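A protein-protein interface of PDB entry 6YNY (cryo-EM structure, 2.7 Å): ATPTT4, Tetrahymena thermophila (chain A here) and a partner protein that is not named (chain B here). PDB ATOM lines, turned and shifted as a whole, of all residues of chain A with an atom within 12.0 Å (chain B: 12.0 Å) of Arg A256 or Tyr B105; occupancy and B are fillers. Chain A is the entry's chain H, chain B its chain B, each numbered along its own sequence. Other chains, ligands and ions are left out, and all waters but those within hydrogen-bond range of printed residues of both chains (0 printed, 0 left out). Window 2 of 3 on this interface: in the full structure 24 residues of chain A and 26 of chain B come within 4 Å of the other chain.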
ATOM      1  N   ASP A 245     -23.050  -5.268 -24.950  1.00  0.00           N
ATOM      2  CA  ASP A 245     -23.413  -6.002 -23.752  1.00  0.00           C
ATOM      3  C   ASP A 245     -23.908  -5.030 -22.689  1.00  0.00           C
ATOM      4  O   ASP A 245     -23.710  -3.816 -22.778  1.00  0.00           O
ATOM      5  CB  ASP A 245     -22.222  -6.794 -23.223  1.00  0.00           C
ATOM      6  CG  ASP A 245     -21.620  -7.700 -24.270  1.00  0.00           C
ATOM      7  OD1 ASP A 245     -22.186  -7.776 -25.380  1.00  0.00           O
ATOM      8  OD2 ASP A 245     -20.579  -8.330 -23.986  1.00  0.00           O
ATOM      9  N   ASN A 247     -22.690  -4.567 -19.972  1.00  0.00           N
ATOM     10  CA  ASN A 247     -21.561  -4.042 -19.225  1.00  0.00           C
ATOM     11  C   ASN A 247     -21.269  -2.600 -19.623  1.00  0.00           C
ATOM     12  O   ASN A 247     -21.493  -2.185 -20.762  1.00  0.00           O
ATOM     13  CB  ASN A 247     -20.332  -4.911 -19.463  1.00  0.00           C
ATOM     14  CG  ASN A 247     -20.519  -6.324 -18.971  1.00  0.00           C
ATOM     15  OD1 ASN A 247     -21.625  -6.733 -18.623  1.00  0.00           O
ATOM     16  ND2 ASN A 247     -19.434  -7.084 -18.943  1.00  0.00           N
ATOM     17  N   VAL A 248     -20.759  -1.836 -18.658  1.00  0.00           N
ATOM     18  CA  VAL A 248     -20.401  -0.447 -18.905  1.00  0.00           C
ATOM     19  C   VAL A 248     -19.112  -0.376 -19.715  1.00  0.00           C
ATOM     20  O   VAL A 248     -18.238  -1.249 -19.625  1.00  0.00           O
ATOM     21  CB  VAL A 248     -20.276   0.303 -17.568  1.00  0.00           C
ATOM     22  CG1 VAL A 248     -19.886   1.742 -17.786  1.00  0.00           C
ATOM     23  CG2 VAL A 248     -21.578   0.233 -16.815  1.00  0.00           C
ATOM     24  N   ASP A 250     -16.636   1.792 -19.546  1.00  0.00           N
ATOM     25  CA  ASP A 250     -15.614   2.618 -18.930  1.00  0.00           C
ATOM     26  C   ASP A 250     -14.316   1.840 -18.746  1.00  0.00           C
ATOM     27  O   ASP A 250     -14.259   0.618 -18.896  1.00  0.00           O
ATOM     28  CB  ASP A 250     -16.105   3.143 -17.586  1.00  0.00           C
ATOM     29  CG  ASP A 250     -17.349   3.983 -17.717  1.00  0.00           C
ATOM     30  OD1 ASP A 250     -17.519   4.634 -18.768  1.00  0.00           O
ATOM     31  OD2 ASP A 250     -18.160   3.992 -16.767  1.00  0.00           O
ATOM     32  N   PHE A 251     -13.256   2.579 -18.422  1.00  0.00           N
ATOM     33  CA  PHE A 251     -11.972   1.974 -18.101  1.00  0.00           C
ATOM     34  C   PHE A 251     -12.003   1.212 -16.786  1.00  0.00           C
ATOM     35  O   PHE A 251     -11.076   0.443 -16.511  1.00  0.00           O
ATOM     36  CB  PHE A 251     -10.892   3.053 -18.048  1.00  0.00           C
ATOM     37  CG  PHE A 251     -11.012   3.980 -16.876  1.00  0.00           C
ATOM     38  CD1 PHE A 251     -10.216   3.813 -15.761  1.00  0.00           C
ATOM     39  CD2 PHE A 251     -11.919   5.020 -16.887  1.00  0.00           C
ATOM     40  CE1 PHE A 251     -10.323   4.662 -14.687  1.00  0.00           C
ATOM     41  CE2 PHE A 251     -12.030   5.868 -15.814  1.00  0.00           C
ATOM     42  CZ  PHE A 251     -11.230   5.689 -14.713  1.00  0.00           C
ATOM     43  N   LEU A 252     -13.040   1.405 -15.975  1.00  0.00           N
ATOM     44  CA  LEU A 252     -13.173   0.709 -14.706  1.00  0.00           C
ATOM     45  C   LEU A 252     -13.850  -0.647 -14.837  1.00  0.00           C
ATOM     46  O   LEU A 252     -13.774  -1.451 -13.903  1.00  0.00           O
ATOM     47  CB  LEU A 252     -13.971   1.564 -13.722  1.00  0.00           C
ATOM     48  CG  LEU A 252     -13.379   2.929 -13.402  1.00  0.00           C
ATOM     49  CD1 LEU A 252     -14.391   3.788 -12.686  1.00  0.00           C
ATOM     50  CD2 LEU A 252     -12.134   2.764 -12.571  1.00  0.00           C
ATOM     51  N   GLU A 253     -14.506  -0.919 -15.961  1.00  0.00           N
ATOM     52  CA  GLU A 253     -15.233  -2.172 -16.145  1.00  0.00           C
ATOM     53  C   GLU A 253     -14.315  -3.267 -16.671  1.00  0.00           C
ATOM     54  O   GLU A 253     -14.566  -3.892 -17.701  1.00  0.00           O
ATOM     55  CB  GLU A 253     -16.418  -1.953 -17.076  1.00  0.00           C
ATOM     56  CG  GLU A 253     -17.386  -3.127 -17.144  1.00  0.00           C
ATOM     57  CD  GLU A 253     -18.050  -3.406 -15.818  1.00  0.00           C
ATOM     58  OE1 GLU A 253     -18.000  -2.526 -14.934  1.00  0.00           O
ATOM     59  OE2 GLU A 253     -18.619  -4.507 -15.660  1.00  0.00           O
ATOM     60  N   GLN A 254     -13.223  -3.491 -15.954  1.00  0.00           N
ATOM     61  CA  GLN A 254     -12.312  -4.598 -16.207  1.00  0.00           C
ATOM     62  C   GLN A 254     -12.403  -5.547 -15.020  1.00  0.00           C
ATOM     63  O   GLN A 254     -11.802  -5.304 -13.970  1.00  0.00           O
ATOM     64  CB  GLN A 254     -10.885  -4.108 -16.422  1.00  0.00           C
ATOM     65  CG  GLN A 254     -10.349  -4.409 -17.804  1.00  0.00           C
ATOM     66  CD  GLN A 254     -10.359  -5.893 -18.120  1.00  0.00           C
ATOM     67  OE1 GLN A 254     -10.687  -6.718 -17.269  1.00  0.00           O
ATOM     68  NE2 GLN A 254     -10.008  -6.239 -19.351  1.00  0.00           N
ATOM     69  N   ARG A 255     -13.161  -6.621 -15.189  1.00  0.00           N
ATOM     70  CA  ARG A 255     -13.367  -7.600 -14.142  1.00  0.00           C
ATOM     71  C   ARG A 255     -12.488  -8.813 -14.408  1.00  0.00           C
ATOM     72  O   ARG A 255     -11.686  -8.843 -15.343  1.00  0.00           O
ATOM     73  CB  ARG A 255     -14.835  -8.022 -14.069  1.00  0.00           C
ATOM     74  CG  ARG A 255     -15.853  -6.910 -14.186  1.00  0.00           C
ATOM     75  CD  ARG A 255     -15.721  -5.889 -13.088  1.00  0.00           C
ATOM     76  NE  ARG A 255     -16.719  -4.833 -13.207  1.00  0.00           N
ATOM     77  CZ  ARG A 255     -17.975  -4.947 -12.789  1.00  0.00           C
ATOM     78  NH1 ARG A 255     -18.393  -6.065 -12.227  1.00  0.00           N
ATOM     79  NH2 ARG A 255     -18.818  -3.941 -12.930  1.00  0.00           N
ATOM     80  N   ARG A 256     -12.638  -9.828 -13.566  1.00  0.00           N
ATOM     81  CA  ARG A 256     -11.989 -11.090 -13.827  1.00  0.00           C
ATOM     82  C   ARG A 256     -12.470 -11.644 -15.166  1.00  0.00           C
ATOM     83  O   ARG A 256     -13.543 -11.276 -15.649  1.00  0.00           O
ATOM     84  CB  ARG A 256     -12.283 -12.085 -12.715  1.00  0.00           C
ATOM     85  CG  ARG A 256     -11.439 -11.920 -11.475  1.00  0.00           C
ATOM     86  CD  ARG A 256     -10.991 -13.265 -10.955  1.00  0.00           C
ATOM     87  NE  ARG A 256     -10.966 -13.326  -9.506  1.00  0.00           N
ATOM     88  CZ  ARG A 256     -10.608 -14.403  -8.819  1.00  0.00           C
ATOM     89  NH1 ARG A 256     -10.240 -15.504  -9.453  1.00  0.00           N
ATOM     90  NH2 ARG A 256     -10.620 -14.379  -7.499  1.00  0.00           N
ATOM     91  N   PRO A 257     -11.693 -12.542 -15.785  1.00  0.00           N
ATOM     92  CA  PRO A 257     -10.420 -13.076 -15.295  1.00  0.00           C
ATOM     93  C   PRO A 257      -9.240 -12.120 -15.429  1.00  0.00           C
ATOM     94  O   PRO A 257      -9.218 -11.257 -16.305  1.00  0.00           O
ATOM     95  CB  PRO A 257     -10.211 -14.312 -16.168  1.00  0.00           C
ATOM     96  CG  PRO A 257     -10.927 -14.017 -17.409  1.00  0.00           C
ATOM     97  CD  PRO A 257     -12.123 -13.216 -17.019  1.00  0.00           C
ATOM     98  N   PHE A 258      -8.262 -12.290 -14.543  1.00  0.00           N
ATOM     99  CA  PHE A 258      -7.065 -11.463 -14.537  1.00  0.00           C
ATOM    100  C   PHE A 258      -6.057 -12.007 -15.538  1.00  0.00           C
ATOM    101  O   PHE A 258      -5.629 -13.161 -15.432  1.00  0.00           O
ATOM    102  CB  PHE A 258      -6.451 -11.430 -13.140  1.00  0.00           C
ATOM    103  CG  PHE A 258      -7.306 -10.762 -12.105  1.00  0.00           C
ATOM    104  CD1 PHE A 258      -7.993  -9.600 -12.389  1.00  0.00           C
ATOM    105  CD2 PHE A 258      -7.408 -11.294 -10.837  1.00  0.00           C
ATOM    106  CE1 PHE A 258      -8.765  -8.991 -11.431  1.00  0.00           C
ATOM    107  CE2 PHE A 258      -8.178 -10.689  -9.880  1.00  0.00           C
ATOM    108  CZ  PHE A 258      -8.857  -9.535 -10.178  1.00  0.00           C
ATOM    109  N   GLU A 259      -5.677 -11.176 -16.507  1.00  0.00           N
ATOM    110  CA  GLU A 259      -4.736 -11.587 -17.535  1.00  0.00           C
ATOM    111  C   GLU A 259      -3.688 -10.530 -17.853  1.00  0.00           C
ATOM    112  O   GLU A 259      -2.878 -10.748 -18.758  1.00  0.00           O
ATOM    113  CB  GLU A 259      -5.492 -11.956 -18.820  1.00  0.00           C
ATOM    114  CG  GLU A 259      -6.512 -13.061 -18.631  1.00  0.00           C
ATOM    115  CD  GLU A 259      -7.297 -13.357 -19.890  1.00  0.00           C
ATOM    116  OE1 GLU A 259      -7.161 -12.595 -20.871  1.00  0.00           O
ATOM    117  OE2 GLU A 259      -8.052 -14.351 -19.899  1.00  0.00           O
ATOM    118  N   HIS A 260      -3.670  -9.405 -17.143  1.00  0.00           N
ATOM    119  CA  HIS A 260      -2.723  -8.327 -17.390  1.00  0.00           C
ATOM    120  C   HIS A 260      -1.558  -8.420 -16.419  1.00  0.00           C
ATOM    121  O   HIS A 260      -1.781  -8.579 -15.211  1.00  0.00           O
ATOM    122  CB  HIS A 260      -3.404  -6.971 -17.247  1.00  0.00           C
ATOM    123  CG  HIS A 260      -4.338  -6.647 -18.369  1.00  0.00           C
ATOM    124  ND1 HIS A 260      -4.037  -5.716 -19.339  1.00  0.00           N
ATOM    125  CD2 HIS A 260      -5.561  -7.135 -18.681  1.00  0.00           C
ATOM    126  CE1 HIS A 260      -5.038  -5.641 -20.198  1.00  0.00           C
ATOM    127  NE2 HIS A 260      -5.975  -6.492 -19.822  1.00  0.00           N
ATOM    128  N   GLN B 100     -14.668   2.797  -7.127  1.00  0.00           N
ATOM    129  CA  GLN B 100     -13.759   1.686  -6.860  1.00  0.00           C
ATOM    130  C   GLN B 100     -14.468   0.385  -7.215  1.00  0.00           C
ATOM    131  O   GLN B 100     -15.060  -0.297  -6.376  1.00  0.00           O
ATOM    132  CB  GLN B 100     -13.299   1.700  -5.411  1.00  0.00           C
ATOM    133  CG  GLN B 100     -12.604   2.978  -5.027  1.00  0.00           C
ATOM    134  CD  GLN B 100     -11.734   2.833  -3.809  1.00  0.00           C
ATOM    135  OE1 GLN B 100     -11.740   1.803  -3.141  1.00  0.00           O
ATOM    136  NE2 GLN B 100     -10.971   3.868  -3.515  1.00  0.00           N
ATOM    137  N   VAL B 101     -14.403   0.047  -8.494  1.00  0.00           N
ATOM    138  CA  VAL B 101     -15.052  -1.150  -9.008  1.00  0.00           C
ATOM    139  C   VAL B 101     -14.247  -2.370  -8.596  1.00  0.00           C
ATOM    140  O   VAL B 101     -13.036  -2.443  -8.834  1.00  0.00           O
ATOM    141  CB  VAL B 101     -15.200  -1.068 -10.534  1.00  0.00           C
ATOM    142  CG1 VAL B 101     -15.785  -2.344 -11.080  1.00  0.00           C
ATOM    143  CG2 VAL B 101     -16.063   0.110 -10.911  1.00  0.00           C
ATOM    144  N   SER B 102     -14.918  -3.327  -7.968  1.00  0.00           N
ATOM    145  CA  SER B 102     -14.288  -4.578  -7.590  1.00  0.00           C
ATOM    146  C   SER B 102     -14.336  -5.546  -8.761  1.00  0.00           C
ATOM    147  O   SER B 102     -15.428  -5.817  -9.277  1.00  0.00           O
ATOM    148  CB  SER B 102     -14.980  -5.186  -6.389  1.00  0.00           C
ATOM    149  OG  SER B 102     -14.425  -6.444  -6.060  1.00  0.00           O
ATOM    150  N   PRO B 103     -13.202  -6.076  -9.221  1.00  0.00           N
ATOM    151  CA  PRO B 103     -13.225  -7.058 -10.307  1.00  0.00           C
ATOM    152  C   PRO B 103     -13.479  -8.482  -9.851  1.00  0.00           C
ATOM    153  O   PRO B 103     -13.468  -9.392 -10.686  1.00  0.00           O
ATOM    154  CB  PRO B 103     -11.821  -6.921 -10.897  1.00  0.00           C
ATOM    155  CG  PRO B 103     -10.986  -6.584  -9.737  1.00  0.00           C
ATOM    156  CD  PRO B 103     -11.823  -5.739  -8.831  1.00  0.00           C
ATOM    157  N   HIS B 104     -13.712  -8.697  -8.566  1.00  0.00           N
ATOM    158  CA  HIS B 104     -13.768 -10.032  -8.006  1.00  0.00           C
ATOM    159  C   HIS B 104     -15.154 -10.647  -8.138  1.00  0.00           C
ATOM    160  O   HIS B 104     -16.141  -9.985  -8.463  1.00  0.00           O
ATOM    161  CB  HIS B 104     -13.356 -10.009  -6.538  1.00  0.00           C
ATOM    162  CG  HIS B 104     -11.912  -9.697  -6.318  1.00  0.00           C
ATOM    163  ND1 HIS B 104     -11.436  -8.410  -6.201  1.00  0.00           N
ATOM    164  CD2 HIS B 104     -10.838 -10.508  -6.191  1.00  0.00           C
ATOM    165  CE1 HIS B 104     -10.131  -8.443  -6.010  1.00  0.00           C
ATOM    166  NE2 HIS B 104      -9.743  -9.704  -6.000  1.00  0.00           N
ATOM    167  N   TYR B 105     -15.207 -11.948  -7.869  1.00  0.00           N
ATOM    168  CA  TYR B 105     -16.452 -12.695  -7.885  1.00  0.00           C
ATOM    169  C   TYR B 105     -17.206 -12.604  -6.572  1.00  0.00           C
ATOM    170  O   TYR B 105     -18.404 -12.902  -6.541  1.00  0.00           O
ATOM    171  CB  TYR B 105     -16.159 -14.157  -8.197  1.00  0.00           C
ATOM    172  CG  TYR B 105     -15.483 -14.381  -9.524  1.00  0.00           C
ATOM    173  CD1 TYR B 105     -15.856 -13.663 -10.645  1.00  0.00           C
ATOM    174  CD2 TYR B 105     -14.467 -15.309  -9.655  1.00  0.00           C
ATOM    175  CE1 TYR B 105     -15.245 -13.867 -11.852  1.00  0.00           C
ATOM    176  CE2 TYR B 105     -13.850 -15.517 -10.859  1.00  0.00           C
ATOM    177  CZ  TYR B 105     -14.240 -14.792 -11.956  1.00  0.00           C
ATOM    178  OH  TYR B 105     -13.625 -14.998 -13.163  1.00  0.00           O
ATOM    179  N   GLU B 106     -16.540 -12.207  -5.494  1.00  0.00           N
ATOM    180  CA  GLU B 106     -17.169 -12.091  -4.192  1.00  0.00           C
ATOM    181  C   GLU B 106     -16.697 -10.818  -3.514  1.00  0.00           C
ATOM    182  O   GLU B 106     -15.604 -10.318  -3.786  1.00  0.00           O
ATOM    183  CB  GLU B 106     -16.861 -13.298  -3.301  1.00  0.00           C
ATOM    184  CG  GLU B 106     -15.380 -13.598  -3.133  1.00  0.00           C
ATOM    185  CD  GLU B 106     -14.782 -14.315  -4.321  1.00  0.00           C
ATOM    186  OE1 GLU B 106     -15.414 -15.267  -4.823  1.00  0.00           O
ATOM    187  OE2 GLU B 106     -13.680 -13.926  -4.759  1.00  0.00           O
ATOM    188  N   SER B 107     -17.537 -10.300  -2.627  1.00  0.00           N
ATOM    189  CA  SER B 107     -17.209  -9.084  -1.909  1.00  0.00           C
ATOM    190  C   SER B 107     -16.064  -9.333  -0.932  1.00  0.00           C
ATOM    191  O   SER B 107     -15.808 -10.458  -0.497  1.00  0.00           O
ATOM    192  CB  SER B 107     -18.439  -8.551  -1.180  1.00  0.00           C
ATOM    193  OG  SER B 107     -19.208  -9.604  -0.638  1.00  0.00           O
ATOM    194  N   PHE B 108     -15.370  -8.249  -0.587  1.00  0.00           N
ATOM    195  CA  PHE B 108     -14.163  -8.364   0.223  1.00  0.00           C
ATOM    196  C   PHE B 108     -14.472  -8.804   1.648  1.00  0.00           C
ATOM    197  O   PHE B 108     -13.734  -9.609   2.225  1.00  0.00           O
ATOM    198  CB  PHE B 108     -13.419  -7.034   0.220  1.00  0.00           C
ATOM    199  CG  PHE B 108     -12.299  -6.965   1.204  1.00  0.00           C
ATOM    200  CD1 PHE B 108     -11.233  -7.834   1.126  1.00  0.00           C
ATOM    201  CD2 PHE B 108     -12.306  -6.016   2.202  1.00  0.00           C
ATOM    202  CE1 PHE B 108     -10.209  -7.764   2.028  1.00  0.00           C
ATOM    203  CE2 PHE B 108     -11.284  -5.944   3.105  1.00  0.00           C
ATOM    204  CZ  PHE B 108     -10.232  -6.818   3.019  1.00  0.00           C
ATOM    205  N   ALA B 109     -15.554  -8.295   2.230  1.00  0.00           N
ATOM    206  CA  ALA B 109     -15.858  -8.608   3.622  1.00  0.00           C
ATOM    207  C   ALA B 109     -16.272 -10.063   3.787  1.00  0.00           C
ATOM    208  O   ALA B 109     -15.773 -10.766   4.671  1.00  0.00           O
ATOM    209  CB  ALA B 109     -16.950  -7.677   4.141  1.00  0.00           C
ATOM    210  N   MET B 110     -17.188 -10.535   2.941  1.00  0.00           N
ATOM    211  CA  MET B 110     -17.642 -11.917   3.040  1.00  0.00           C
ATOM    212  C   MET B 110     -16.502 -12.905   2.840  1.00  0.00           C
ATOM    213  O   MET B 110     -16.556 -14.024   3.360  1.00  0.00           O
ATOM    214  CB  MET B 110     -18.737 -12.174   2.013  1.00  0.00           C
ATOM    215  CG  MET B 110     -18.254 -12.068   0.593  1.00  0.00           C
ATOM    216  SD  MET B 110     -19.544 -12.319  -0.629  1.00  0.00           S
ATOM    217  CE  MET B 110     -19.696 -14.094  -0.534  1.00  0.00           C
ATOM    218  N   SER B 111     -15.474 -12.521   2.090  1.00  0.00           N
ATOM    219  CA  SER B 111     -14.344 -13.405   1.843  1.00  0.00           C
ATOM    220  C   SER B 111     -13.309 -13.369   2.957  1.00  0.00           C
ATOM    221  O   SER B 111     -12.432 -14.238   2.990  1.00  0.00           O
ATOM    222  CB  SER B 111     -13.676 -13.035   0.521  1.00  0.00           C
ATOM    223  OG  SER B 111     -13.037 -11.778   0.608  1.00  0.00           O
ATOM    224  N   ARG B 112     -13.390 -12.398   3.866  1.00  0.00           N
ATOM    225  CA  ARG B 112     -12.403 -12.220   4.923  1.00  0.00           C
ATOM    226  C   ARG B 112     -13.075 -12.003   6.273  1.00  0.00           C
ATOM    227  O   ARG B 112     -12.555 -11.274   7.119  1.00  0.00           O
ATOM    228  CB  ARG B 112     -11.474 -11.053   4.599  1.00  0.00           C
ATOM    229  CG  ARG B 112     -10.830 -11.123   3.234  1.00  0.00           C
ATOM    230  CD  ARG B 112      -9.727 -12.141   3.176  1.00  0.00           C
ATOM    231  NE  ARG B 112      -9.210 -12.327   1.826  1.00  0.00           N
ATOM    232  CZ  ARG B 112      -7.973 -12.716   1.547  1.00  0.00           C
ATOM    233  NH1 ARG B 112      -7.605 -12.864   0.288  1.00  0.00           N
ATOM    234  NH2 ARG B 112      -7.098 -12.933   2.519  1.00  0.00           N
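O of Pro B103 lies within hydrogen-bond range of N of Arg A256.
The guanidinium group of Arg A255 lies within salt-bridge range of the side-chain carboxylate of Glu A253. The side-chain hydroxyl (OG) of Ser B102 lies close to the backbone NH (N) of His B104 (3.4 Å).
Among the printed residues, merely in contact across the chains: Arg A256 with Tyr B105, Arg A255 with Val B101, Gln A254 with Pro B103, Leu A252 with Val B101, Arg A255 with Pro B103, Phe A258 with Pro B103 and Arg A255 with Ser B102.
Arg A256 touches just these residues of chain B: Pro B103 and Tyr B105. Tyr B105 touches one residue of chain A. Phe A258 touches one residue of chain B. Of the printed residues of chain A, Pro B103 touches Gln A254, Arg A255, Arg A256 and Phe A258. No residue of chain A comes within 4 Å of His B104. No residue of chain A comes within 4 Å of Glu B106. No residue of chain A comes within 4 Å of Ser B107. Printed residues of chain A within 4 Å of Val B101: Leu A252 (3.6 Å) and Arg A255 (3.4 Å). Printed residues of chain A within 4 Å of Ser B102: Arg A255. Printed residues of chain B within 4 Å of Leu A252: Val B101. Of the printed residues of chain B, Arg A255 touches Val B101 (3.4 Å), Ser B102 (3.8 Å) and Pro B103 (3.7 Å). Glu A259 touches none of the printed residues of chain B. Val A248 touches none of the printed residues of chain B. The nearest residue of chain B that does not touch Arg A256 is His B104 (4.1 Å).
Printed residues of chain B that touch a printed residue of chain A: Val B101, Ser B102, Pro B103 and Tyr B105. Printed residues of chain A that touch a printed residue of chain B: Leu A252, Gln A254, Arg A255, Arg A256 and Phe A258. Hydrophobic or aromatic side chains of chain A within 4 Å of the printed part of chain B: Leu A252 and Phe A258. Along chain A the printed residues that touch a printed residue of chain B span positions 252 to 258. Among the printed residues, 8 pairs touch across the chains.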
